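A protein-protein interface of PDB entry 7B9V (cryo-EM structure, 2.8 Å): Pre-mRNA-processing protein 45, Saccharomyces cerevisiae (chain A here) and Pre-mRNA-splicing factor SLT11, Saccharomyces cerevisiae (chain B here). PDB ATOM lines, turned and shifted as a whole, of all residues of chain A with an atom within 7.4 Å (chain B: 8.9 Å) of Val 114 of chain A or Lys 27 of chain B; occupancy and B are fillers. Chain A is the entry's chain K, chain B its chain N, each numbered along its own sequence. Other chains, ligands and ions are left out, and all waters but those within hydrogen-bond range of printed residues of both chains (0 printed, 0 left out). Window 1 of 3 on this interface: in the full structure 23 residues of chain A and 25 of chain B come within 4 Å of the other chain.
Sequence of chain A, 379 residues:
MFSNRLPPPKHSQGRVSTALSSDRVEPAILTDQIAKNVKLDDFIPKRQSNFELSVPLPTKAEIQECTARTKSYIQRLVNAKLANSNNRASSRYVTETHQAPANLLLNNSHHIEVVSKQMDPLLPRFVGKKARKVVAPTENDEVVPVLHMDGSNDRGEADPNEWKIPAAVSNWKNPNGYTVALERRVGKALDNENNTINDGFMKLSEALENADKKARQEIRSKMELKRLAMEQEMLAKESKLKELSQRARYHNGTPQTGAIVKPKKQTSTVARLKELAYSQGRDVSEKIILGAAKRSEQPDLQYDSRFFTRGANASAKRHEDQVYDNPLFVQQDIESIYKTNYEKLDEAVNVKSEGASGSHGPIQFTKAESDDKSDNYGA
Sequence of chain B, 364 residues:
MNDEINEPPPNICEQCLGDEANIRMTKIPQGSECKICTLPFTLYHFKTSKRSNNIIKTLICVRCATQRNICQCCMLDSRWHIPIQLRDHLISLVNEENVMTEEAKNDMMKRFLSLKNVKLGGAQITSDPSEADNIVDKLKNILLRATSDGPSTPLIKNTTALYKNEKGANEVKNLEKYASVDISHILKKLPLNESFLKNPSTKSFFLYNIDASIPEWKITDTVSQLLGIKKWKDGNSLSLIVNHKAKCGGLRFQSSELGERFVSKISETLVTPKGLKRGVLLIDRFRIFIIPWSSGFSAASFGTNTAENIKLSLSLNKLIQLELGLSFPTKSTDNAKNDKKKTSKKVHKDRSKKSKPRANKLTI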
ATOM      1  N   ALA A 102      29.650  23.200  17.070  1.00  0.00           N
ATOM      2  CA  ALA A 102      29.910  24.635  17.029  1.00  0.00           C
ATOM      3  C   ALA A 102      28.632  25.436  16.781  1.00  0.00           C
ATOM      4  O   ALA A 102      28.667  26.665  16.732  1.00  0.00           O
ATOM      5  CB  ALA A 102      30.949  24.952  15.963  1.00  0.00           C
ATOM      6  N   ASN A 103      27.504  24.744  16.623  1.00  0.00           N
ATOM      7  CA  ASN A 103      26.218  25.392  16.401  1.00  0.00           C
ATOM      8  C   ASN A 103      25.194  24.838  17.380  1.00  0.00           C
ATOM      9  O   ASN A 103      25.201  23.641  17.683  1.00  0.00           O
ATOM     10  CB  ASN A 103      25.720  25.185  14.970  1.00  0.00           C
ATOM     11  CG  ASN A 103      26.607  25.850  13.951  1.00  0.00           C
ATOM     12  OD1 ASN A 103      26.569  27.067  13.774  1.00  0.00           O
ATOM     13  ND2 ASN A 103      27.411  25.052  13.262  1.00  0.00           N
ATOM     14  N   LEU A 104      24.296  25.707  17.844  1.00  0.00           N
ATOM     15  CA  LEU A 104      23.216  25.331  18.748  1.00  0.00           C
ATOM     16  C   LEU A 104      21.990  26.180  18.447  1.00  0.00           C
ATOM     17  O   LEU A 104      22.099  27.290  17.919  1.00  0.00           O
ATOM     18  CB  LEU A 104      23.593  25.499  20.233  1.00  0.00           C
ATOM     19  CG  LEU A 104      24.758  24.730  20.873  1.00  0.00           C
ATOM     20  CD1 LEU A 104      25.066  25.255  22.273  1.00  0.00           C
ATOM     21  CD2 LEU A 104      24.455  23.247  20.926  1.00  0.00           C
ATOM     22  N   HIS A 111      19.916  31.202  16.715  1.00  0.00           N
ATOM     23  CA  HIS A 111      21.043  30.411  16.238  1.00  0.00           C
ATOM     24  C   HIS A 111      22.315  30.909  16.913  1.00  0.00           C
ATOM     25  O   HIS A 111      22.631  32.103  16.860  1.00  0.00           O
ATOM     26  CB  HIS A 111      21.165  30.509  14.717  1.00  0.00           C
ATOM     27  CG  HIS A 111      22.398  29.866  14.157  1.00  0.00           C
ATOM     28  ND1 HIS A 111      22.485  28.508  13.938  1.00  0.00           N
ATOM     29  CD2 HIS A 111      23.588  30.386  13.776  1.00  0.00           C
ATOM     30  CE1 HIS A 111      23.671  28.221  13.434  1.00  0.00           C
ATOM     31  NE2 HIS A 111      24.363  29.342  13.331  1.00  0.00           N
ATOM     32  N   ILE A 112      23.035  29.993  17.549  1.00  0.00           N
ATOM     33  CA  ILE A 112      24.178  30.319  18.390  1.00  0.00           C
ATOM     34  C   ILE A 112      25.439  29.747  17.755  1.00  0.00           C
ATOM     35  O   ILE A 112      25.514  28.543  17.481  1.00  0.00           O
ATOM     36  CB  ILE A 112      23.979  29.775  19.817  1.00  0.00           C
ATOM     37  CG1 ILE A 112      22.664  30.276  20.432  1.00  0.00           C
ATOM     38  CG2 ILE A 112      25.138  30.131  20.685  1.00  0.00           C
ATOM     39  CD1 ILE A 112      22.499  31.784  20.421  1.00  0.00           C
ATOM     40  N   GLU A 113      26.427  30.613  17.535  1.00  0.00           N
ATOM     41  CA  GLU A 113      27.753  30.213  17.078  1.00  0.00           C
ATOM     42  C   GLU A 113      28.642  30.030  18.303  1.00  0.00           C
ATOM     43  O   GLU A 113      28.988  31.006  18.978  1.00  0.00           O
ATOM     44  CB  GLU A 113      28.317  31.270  16.130  1.00  0.00           C
ATOM     45  CG  GLU A 113      29.760  31.072  15.676  1.00  0.00           C
ATOM     46  CD  GLU A 113      29.930  29.908  14.716  1.00  0.00           C
ATOM     47  OE1 GLU A 113      29.267  29.906  13.657  1.00  0.00           O
ATOM     48  OE2 GLU A 113      30.750  29.010  15.002  1.00  0.00           O
ATOM     49  N   VAL A 114      29.005  28.786  18.595  1.00  0.00           N
ATOM     50  CA  VAL A 114      29.798  28.467  19.775  1.00  0.00           C
ATOM     51  C   VAL A 114      31.266  28.446  19.383  1.00  0.00           C
ATOM     52  O   VAL A 114      31.682  27.645  18.540  1.00  0.00           O
ATOM     53  CB  VAL A 114      29.372  27.127  20.387  1.00  0.00           C
ATOM     54  CG1 VAL A 114      30.184  26.830  21.640  1.00  0.00           C
ATOM     55  CG2 VAL A 114      27.903  27.167  20.709  1.00  0.00           C
ATOM     56  N   VAL A 115      32.052  29.327  19.996  1.00  0.00           N
ATOM     57  CA  VAL A 115      33.496  29.327  19.850  1.00  0.00           C
ATOM     58  C   VAL A 115      34.114  29.014  21.209  1.00  0.00           C
ATOM     59  O   VAL A 115      33.425  28.899  22.220  1.00  0.00           O
ATOM     60  CB  VAL A 115      34.034  30.657  19.286  1.00  0.00           C
ATOM     61  CG1 VAL A 115      33.581  30.834  17.844  1.00  0.00           C
ATOM     62  CG2 VAL A 115      33.591  31.827  20.143  1.00  0.00           C
ATOM     63  N   SER A 116      35.431  28.833  21.207  1.00  0.00           N
ATOM     64  CA  SER A 116      36.194  28.604  22.433  1.00  0.00           C
ATOM     65  C   SER A 116      37.534  29.309  22.249  1.00  0.00           C
ATOM     66  O   SER A 116      38.425  28.760  21.593  1.00  0.00           O
ATOM     67  CB  SER A 116      36.381  27.117  22.714  1.00  0.00           C
ATOM     68  OG  SER A 116      37.072  26.483  21.653  1.00  0.00           O
ATOM     69  N   LYS A 117      37.645  30.532  22.779  1.00  0.00           N
ATOM     70  CA  LYS A 117      38.797  31.395  22.524  1.00  0.00           C
ATOM     71  C   LYS A 117      40.067  30.811  23.140  1.00  0.00           C
ATOM     72  O   LYS A 117      40.018  30.024  24.089  1.00  0.00           O
ATOM     73  CB  LYS A 117      38.539  32.805  23.068  1.00  0.00           C
ATOM     74  CG  LYS A 117      38.516  32.924  24.592  1.00  0.00           C
ATOM     75  CD  LYS A 117      37.839  34.214  25.049  1.00  0.00           C
ATOM     76  CE  LYS A 117      38.621  35.447  24.629  1.00  0.00           C
ATOM     77  NZ  LYS A 117      37.880  36.691  24.967  1.00  0.00           N
ATOM     78  N   MET A 119      43.186  30.147  25.239  1.00  0.00           N
ATOM     79  CA  MET A 119      43.547  30.520  26.591  1.00  0.00           C
ATOM     80  C   MET A 119      44.986  31.012  26.633  1.00  0.00           C
ATOM     81  O   MET A 119      45.814  30.616  25.807  1.00  0.00           O
ATOM     82  CB  MET A 119      43.387  29.325  27.532  1.00  0.00           C
ATOM     83  CG  MET A 119      42.017  28.679  27.494  1.00  0.00           C
ATOM     84  SD  MET A 119      40.699  29.803  27.985  1.00  0.00           S
ATOM     85  CE  MET A 119      40.918  29.814  29.762  1.00  0.00           C
ATOM     86  N   GLU B   7      26.566  15.892  27.700  1.00  0.00           N
ATOM     87  CA  GLU B   7      26.660  17.127  28.462  1.00  0.00           C
ATOM     88  C   GLU B   7      25.529  18.025  27.968  1.00  0.00           C
ATOM     89  O   GLU B   7      25.451  18.252  26.761  1.00  0.00           O
ATOM     90  CB  GLU B   7      28.014  17.806  28.246  1.00  0.00           C
ATOM     91  CG  GLU B   7      29.214  17.147  28.932  1.00  0.00           C
ATOM     92  CD  GLU B   7      29.749  15.917  28.191  1.00  0.00           C
ATOM     93  OE1 GLU B   7      29.097  14.850  28.216  1.00  0.00           O
ATOM     94  OE2 GLU B   7      30.837  16.022  27.585  1.00  0.00           O
ATOM     95  N   PRO B   8      24.642  18.464  28.866  1.00  0.00           N
ATOM     96  CA  PRO B   8      23.420  19.182  28.428  1.00  0.00           C
ATOM     97  C   PRO B   8      23.730  20.535  27.785  1.00  0.00           C
ATOM     98  O   PRO B   8      24.796  21.116  28.029  1.00  0.00           O
ATOM     99  CB  PRO B   8      22.629  19.347  29.740  1.00  0.00           C
ATOM    100  CG  PRO B   8      23.168  18.296  30.651  1.00  0.00           C
ATOM    101  CD  PRO B   8      24.628  18.226  30.316  1.00  0.00           C
ATOM    102  N   PRO B   9      22.808  21.066  26.977  1.00  0.00           N
ATOM    103  CA  PRO B   9      22.994  22.388  26.384  1.00  0.00           C
ATOM    104  C   PRO B   9      22.684  23.530  27.347  1.00  0.00           C
ATOM    105  O   PRO B   9      21.967  23.319  28.339  1.00  0.00           O
ATOM    106  CB  PRO B   9      22.034  22.374  25.167  1.00  0.00           C
ATOM    107  CG  PRO B   9      20.927  21.547  25.576  1.00  0.00           C
ATOM    108  CD  PRO B   9      21.579  20.460  26.464  1.00  0.00           C
ATOM    109  N   PRO B  10      23.249  24.736  27.116  1.00  0.00           N
ATOM    110  CA  PRO B  10      22.964  25.894  27.987  1.00  0.00           C
ATOM    111  C   PRO B  10      21.482  26.294  27.992  1.00  0.00           C
ATOM    112  O   PRO B  10      20.797  26.220  26.970  1.00  0.00           O
ATOM    113  CB  PRO B  10      23.859  27.019  27.431  1.00  0.00           C
ATOM    114  CG  PRO B  10      24.100  26.688  26.039  1.00  0.00           C
ATOM    115  CD  PRO B  10      24.162  25.143  26.053  1.00  0.00           C
ATOM    116  N   ILE B  23      24.056  35.150  17.378  1.00  0.00           N
ATOM    117  CA  ILE B  23      24.838  35.476  18.565  1.00  0.00           C
ATOM    118  C   ILE B  23      26.056  34.566  18.588  1.00  0.00           C
ATOM    119  O   ILE B  23      25.917  33.338  18.544  1.00  0.00           O
ATOM    120  CB  ILE B  23      24.027  35.372  19.873  1.00  0.00           C
ATOM    121  CG1 ILE B  23      22.973  36.481  19.965  1.00  0.00           C
ATOM    122  CG2 ILE B  23      24.915  35.370  21.101  1.00  0.00           C
ATOM    123  CD1 ILE B  23      21.635  36.140  19.480  1.00  0.00           C
ATOM    124  N   ARG B  24      27.241  35.165  18.645  1.00  0.00           N
ATOM    125  CA  ARG B  24      28.452  34.414  18.931  1.00  0.00           C
ATOM    126  C   ARG B  24      28.573  34.211  20.438  1.00  0.00           C
ATOM    127  O   ARG B  24      28.328  35.130  21.225  1.00  0.00           O
ATOM    128  CB  ARG B  24      29.675  35.135  18.363  1.00  0.00           C
ATOM    129  CG  ARG B  24      30.969  34.343  18.460  1.00  0.00           C
ATOM    130  CD  ARG B  24      32.157  35.165  17.975  1.00  0.00           C
ATOM    131  NE  ARG B  24      32.010  35.624  16.594  1.00  0.00           N
ATOM    132  CZ  ARG B  24      32.178  34.880  15.506  1.00  0.00           C
ATOM    133  NH1 ARG B  24      32.497  33.598  15.578  1.00  0.00           N
ATOM    134  NH2 ARG B  24      32.016  35.440  14.311  1.00  0.00           N
ATOM    135  N   MET B  25      28.949  32.998  20.834  1.00  0.00           N
ATOM    136  CA  MET B  25      29.019  32.598  22.233  1.00  0.00           C
ATOM    137  C   MET B  25      30.323  31.851  22.460  1.00  0.00           C
ATOM    138  O   MET B  25      30.730  31.037  21.630  1.00  0.00           O
ATOM    139  CB  MET B  25      27.823  31.727  22.618  1.00  0.00           C
ATOM    140  CG  MET B  25      27.611  31.513  24.102  1.00  0.00           C
ATOM    141  SD  MET B  25      26.107  30.564  24.367  1.00  0.00           S
ATOM    142  CE  MET B  25      24.877  31.835  24.070  1.00  0.00           C
ATOM    143  N   THR B  26      30.975  32.124  23.586  1.00  0.00           N
ATOM    144  CA  THR B  26      32.260  31.516  23.911  1.00  0.00           C
ATOM    145  C   THR B  26      32.064  30.481  25.006  1.00  0.00           C
ATOM    146  O   THR B  26      31.574  30.801  26.094  1.00  0.00           O
ATOM    147  CB  THR B  26      33.262  32.578  24.361  1.00  0.00           C
ATOM    148  OG1 THR B  26      33.379  33.589  23.352  1.00  0.00           O
ATOM    149  CG2 THR B  26      34.621  31.959  24.631  1.00  0.00           C
ATOM    150  N   LYS B  27      32.465  29.245  24.718  1.00  0.00           N
ATOM    151  CA  LYS B  27      32.387  28.164  25.687  1.00  0.00           C
ATOM    152  C   LYS B  27      33.750  27.954  26.330  1.00  0.00           C
ATOM    153  O   LYS B  27      34.768  27.941  25.634  1.00  0.00           O
ATOM    154  CB  LYS B  27      31.948  26.889  24.969  1.00  0.00           C
ATOM    155  CG  LYS B  27      31.688  25.736  25.869  1.00  0.00           C
ATOM    156  CD  LYS B  27      31.292  24.468  25.141  1.00  0.00           C
ATOM    157  CE  LYS B  27      32.500  23.778  24.526  1.00  0.00           C
ATOM    158  NZ  LYS B  27      32.115  22.474  23.921  1.00  0.00           N
ATOM    159  N   ILE B  28      33.769  27.806  27.659  1.00  0.00           N
ATOM    160  CA  ILE B  28      34.983  27.553  28.447  1.00  0.00           C
ATOM    161  C   ILE B  28      34.687  26.396  29.396  1.00  0.00           C
ATOM    162  O   ILE B  28      33.950  26.611  30.372  1.00  0.00           O
ATOM    163  CB  ILE B  28      35.419  28.807  29.238  1.00  0.00           C
ATOM    164  CG1 ILE B  28      35.411  30.063  28.341  1.00  0.00           C
ATOM    165  CG2 ILE B  28      36.802  28.586  29.858  1.00  0.00           C
ATOM    166  CD1 ILE B  28      36.020  31.272  28.822  1.00  0.00           C
ATOM    167  N   PRO B  29      35.137  25.166  29.115  1.00  0.00           N
ATOM    168  CA  PRO B  29      34.938  24.053  30.062  1.00  0.00           C
ATOM    169  C   PRO B  29      35.635  24.315  31.387  1.00  0.00           C
ATOM    170  O   PRO B  29      36.820  24.656  31.408  1.00  0.00           O
ATOM    171  CB  PRO B  29      35.565  22.861  29.333  1.00  0.00           C
ATOM    172  CG  PRO B  29      35.461  23.204  27.904  1.00  0.00           C
ATOM    173  CD  PRO B  29      35.681  24.693  27.833  1.00  0.00           C
ATOM    174  N   GLN B  30      34.897  24.095  32.486  1.00  0.00           N
ATOM    175  CA  GLN B  30      35.365  24.251  33.879  1.00  0.00           C
ATOM    176  C   GLN B  30      35.960  25.640  34.134  1.00  0.00           C
ATOM    177  O   GLN B  30      36.921  25.803  34.889  1.00  0.00           O
ATOM    178  CB  GLN B  30      36.361  23.152  34.253  1.00  0.00           C
ATOM    179  CG  GLN B  30      35.762  21.759  34.275  1.00  0.00           C
ATOM    180  CD  GLN B  30      36.598  20.794  35.082  1.00  0.00           C
ATOM    181  OE1 GLN B  30      37.821  20.778  34.963  1.00  0.00           O
ATOM    182  NE2 GLN B  30      35.947  19.986  35.913  1.00  0.00           N
ATOM    183  N   GLY B  31      35.379  26.653  33.485  1.00  0.00           N
ATOM    184  CA  GLY B  31      35.885  28.002  33.592  1.00  0.00           C
ATOM    185  C   GLY B  31      35.374  28.792  34.763  1.00  0.00           C
ATOM    186  O   GLY B  31      35.920  29.854  35.066  1.00  0.00           O
ATOM    187  N   PHE B  41      31.854  24.359  36.422  1.00  0.00           N
ATOM    188  CA  PHE B  41      30.981  24.116  35.284  1.00  0.00           C
ATOM    189  C   PHE B  41      31.485  24.825  34.039  1.00  0.00           C
ATOM    190  O   PHE B  41      32.338  25.715  34.082  1.00  0.00           O
ATOM    191  CB  PHE B  41      29.533  24.500  35.617  1.00  0.00           C
ATOM    192  CG  PHE B  41      29.244  25.990  35.621  1.00  0.00           C
ATOM    193  CD1 PHE B  41      29.712  26.803  36.651  1.00  0.00           C
ATOM    194  CD2 PHE B  41      28.471  26.567  34.625  1.00  0.00           C
ATOM    195  CE1 PHE B  41      29.429  28.162  36.676  1.00  0.00           C
ATOM    196  CE2 PHE B  41      28.176  27.925  34.649  1.00  0.00           C
ATOM    197  CZ  PHE B  41      28.659  28.719  35.677  1.00  0.00           C
ATOM    198  N   THR B  42      30.916  24.400  32.920  1.00  0.00           N
ATOM    199  CA  THR B  42      31.188  24.961  31.608  1.00  0.00           C
ATOM    200  C   THR B  42      30.557  26.343  31.473  1.00  0.00           C
ATOM    201  O   THR B  42      29.332  26.479  31.394  1.00  0.00           O
ATOM    202  CB  THR B  42      30.661  23.997  30.550  1.00  0.00           C
ATOM    203  OG1 THR B  42      31.291  22.719  30.704  1.00  0.00           O
ATOM    204  CG2 THR B  42      30.983  24.527  29.203  1.00  0.00           C
ATOM    205  N   LEU B  43      31.401  27.367  31.423  1.00  0.00           N
ATOM    206  CA  LEU B  43      30.961  28.751  31.301  1.00  0.00           C
ATOM    207  C   LEU B  43      30.632  29.093  29.849  1.00  0.00           C
ATOM    208  O   LEU B  43      31.407  28.791  28.939  1.00  0.00           O
ATOM    209  CB  LEU B  43      32.055  29.679  31.821  1.00  0.00           C
ATOM    210  CG  LEU B  43      31.833  31.185  31.757  1.00  0.00           C
ATOM    211  CD1 LEU B  43      30.797  31.639  32.740  1.00  0.00           C
ATOM    212  CD2 LEU B  43      33.117  31.882  32.024  1.00  0.00           C
ATOM    213  N   TYR B  44      29.490  29.735  29.643  1.00  0.00           N
ATOM    214  CA  TYR B  44      29.145  30.382  28.386  1.00  0.00           C
ATOM    215  C   TYR B  44      29.083  31.884  28.619  1.00  0.00           C
ATOM    216  O   TYR B  44      28.541  32.338  29.631  1.00  0.00           O
ATOM    217  CB  TYR B  44      27.821  29.869  27.806  1.00  0.00           C
ATOM    218  CG  TYR B  44      27.853  28.419  27.386  1.00  0.00           C
ATOM    219  CD1 TYR B  44      27.569  27.407  28.296  1.00  0.00           C
ATOM    220  CD2 TYR B  44      28.172  28.067  26.076  1.00  0.00           C
ATOM    221  CE1 TYR B  44      27.582  26.078  27.909  1.00  0.00           C
ATOM    222  CE2 TYR B  44      28.193  26.738  25.679  1.00  0.00           C
ATOM    223  CZ  TYR B  44      27.900  25.750  26.604  1.00  0.00           C
ATOM    224  OH  TYR B  44      27.934  24.429  26.234  1.00  0.00           O
ATOM    225  N   HIS B  45      29.631  32.655  27.675  1.00  0.00           N
ATOM    226  CA  HIS B  45      29.469  34.099  27.730  1.00  0.00           C
ATOM    227  C   HIS B  45      29.382  34.687  26.331  1.00  0.00           C
ATOM    228  O   HIS B  45      29.998  34.191  25.386  1.00  0.00           O
ATOM    229  CB  HIS B  45      30.578  34.790  28.546  1.00  0.00           C
ATOM    230  CG  HIS B  45      31.942  34.767  27.931  1.00  0.00           C
ATOM    231  ND1 HIS B  45      32.318  35.606  26.903  1.00  0.00           N
ATOM    232  CD2 HIS B  45      33.031  34.014  28.216  1.00  0.00           C
ATOM    233  CE1 HIS B  45      33.575  35.370  26.581  1.00  0.00           C
ATOM    234  NE2 HIS B  45      34.030  34.405  27.359  1.00  0.00           N
ATOM    235  N   PHE B  46      28.586  35.752  26.222  1.00  0.00           N
ATOM    236  CA  PHE B  46      28.214  36.336  24.946  1.00  0.00           C
ATOM    237  C   PHE B  46      27.883  37.809  25.139  1.00  0.00           C
ATOM    238  O   PHE B  46      27.686  38.286  26.258  1.00  0.00           O
ATOM    239  CB  PHE B  46      27.002  35.589  24.350  1.00  0.00           C
ATOM    240  CG  PHE B  46      25.722  35.709  25.185  1.00  0.00           C
ATOM    241  CD1 PHE B  46      25.508  34.859  26.272  1.00  0.00           C
ATOM    242  CD2 PHE B  46      24.743  36.651  24.878  1.00  0.00           C
ATOM    243  CE1 PHE B  46      24.365  34.956  27.034  1.00  0.00           C
ATOM    244  CE2 PHE B  46      23.597  36.753  25.646  1.00  0.00           C
ATOM    245  CZ  PHE B  46      23.411  35.903  26.724  1.00  0.00           C
ATOM    246  N   THR B  58      26.931  33.057  31.922  1.00  0.00           N
ATOM    247  CA  THR B  58      26.203  32.115  32.778  1.00  0.00           C
ATOM    248  C   THR B  58      26.797  32.083  34.182  1.00  0.00           C
ATOM    249  O   THR B  58      27.962  31.730  34.370  1.00  0.00           O
ATOM    250  CB  THR B  58      26.243  30.700  32.186  1.00  0.00           C
ATOM    251  OG1 THR B  58      27.597  30.292  31.980  1.00  0.00           O
ATOM    252  CG2 THR B  58      25.495  30.626  30.858  1.00  0.00           C
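N of Val 115 of chain A is in hydrogen-bond range of O of Met 25 of chain B (2.7 Å). The backbone NH (N) of Lys 27 of chain B is in hydrogen-bond range of the backbone carbonyl oxygen (O) of Val 115 of chain A, 2.7 Å away. O of His 111 of chain A lies within hydrogen-bond range of N of Ile 23 of chain B, 3.4 Å away. N of Glu 113 of chain A lies within hydrogen-bond range of O of Ile 23 of chain B (3.0 Å). O of Glu 113 of chain A sits at hydrogen-bond distance from N of Met 25 of chain B (2.7 Å).
NE2 of His 111 of chain A sits close to OD1 of Asn 103 of chain A, at 3.2 Å. The backbone carbonyl oxygen of Ala 102 of chain A sits at hydrogen-bond distance from the backbone NH of Val 114 of chain A (2.8 Å). The backbone NH (N) of Thr 26 of chain B sits at hydrogen-bond distance from the backbone carbonyl oxygen (O) of His 45 of chain B (2.9 Å). O of Leu 104 of chain A sits at hydrogen-bond distance from N of Ile 112 of chain A (2.9 Å).
CD1 of Leu 104 of chain A touches CD of Pro 10 of chain B (3.9 Å). Ile 112 of chain A touches Ile 23 of chain B. Met 25 of chain B touches Ile 112 of chain A. Arg 24 of chain B touches Glu 113 of chain A (CA to O, 3.5 Å). Met 25 of chain B touches Val 114 of chain A (O to CA, 3.3 Å). CG1 of Val 114 of chain A touches CB of Lys 27 of chain B (3.8 Å). Val 115 of chain A touches Arg 24 of chain B. Thr 26 of chain B touches Val 115 of chain A. Ser 116 of chain A touches Lys 27 of chain B (CB to O, 3.4 Å). Lys 117 of chain A touches Thr 26 of chain B (N to CG2, 3.8 Å).
Asn 103 of chain A touches none of the printed residues of chain B. Of the printed residues of chain B, Glu 113 of chain A touches Ile 23 (3.0 Å), Arg 24 (3.5 Å) and Met 25 (2.7 Å). Of chain B, only Met 25 (3.3 Å) and Lys 27 (3.8 Å) come within 4 Å of Val 114 of chain A. Printed residues of chain A within 4 Å of Pro 10 of chain B: Leu 104 (3.9 Å). Lys 27 of chain B touches just these residues of chain A: Val 114 (3.8 Å), Val 115 (2.7 Å) and Ser 116 (3.4 Å). The nearest residue of chain B that does not touch Val 114 of chain A is Tyr 44 of chain B (4.5 Å). The nearest printed residue of chain B that does not touch His 111 of chain A is Arg 24 of chain B (5.8 Å).
Of the 11 printed residues of chain A, 8 touch a printed residue of chain B. Printed residues of chain B that touch a printed residue of chain A: Pro 10, Ile 23, Arg 24, Met 25, Thr 26 and Lys 27. Among the printed residues, 15 pairs touch across the chains.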
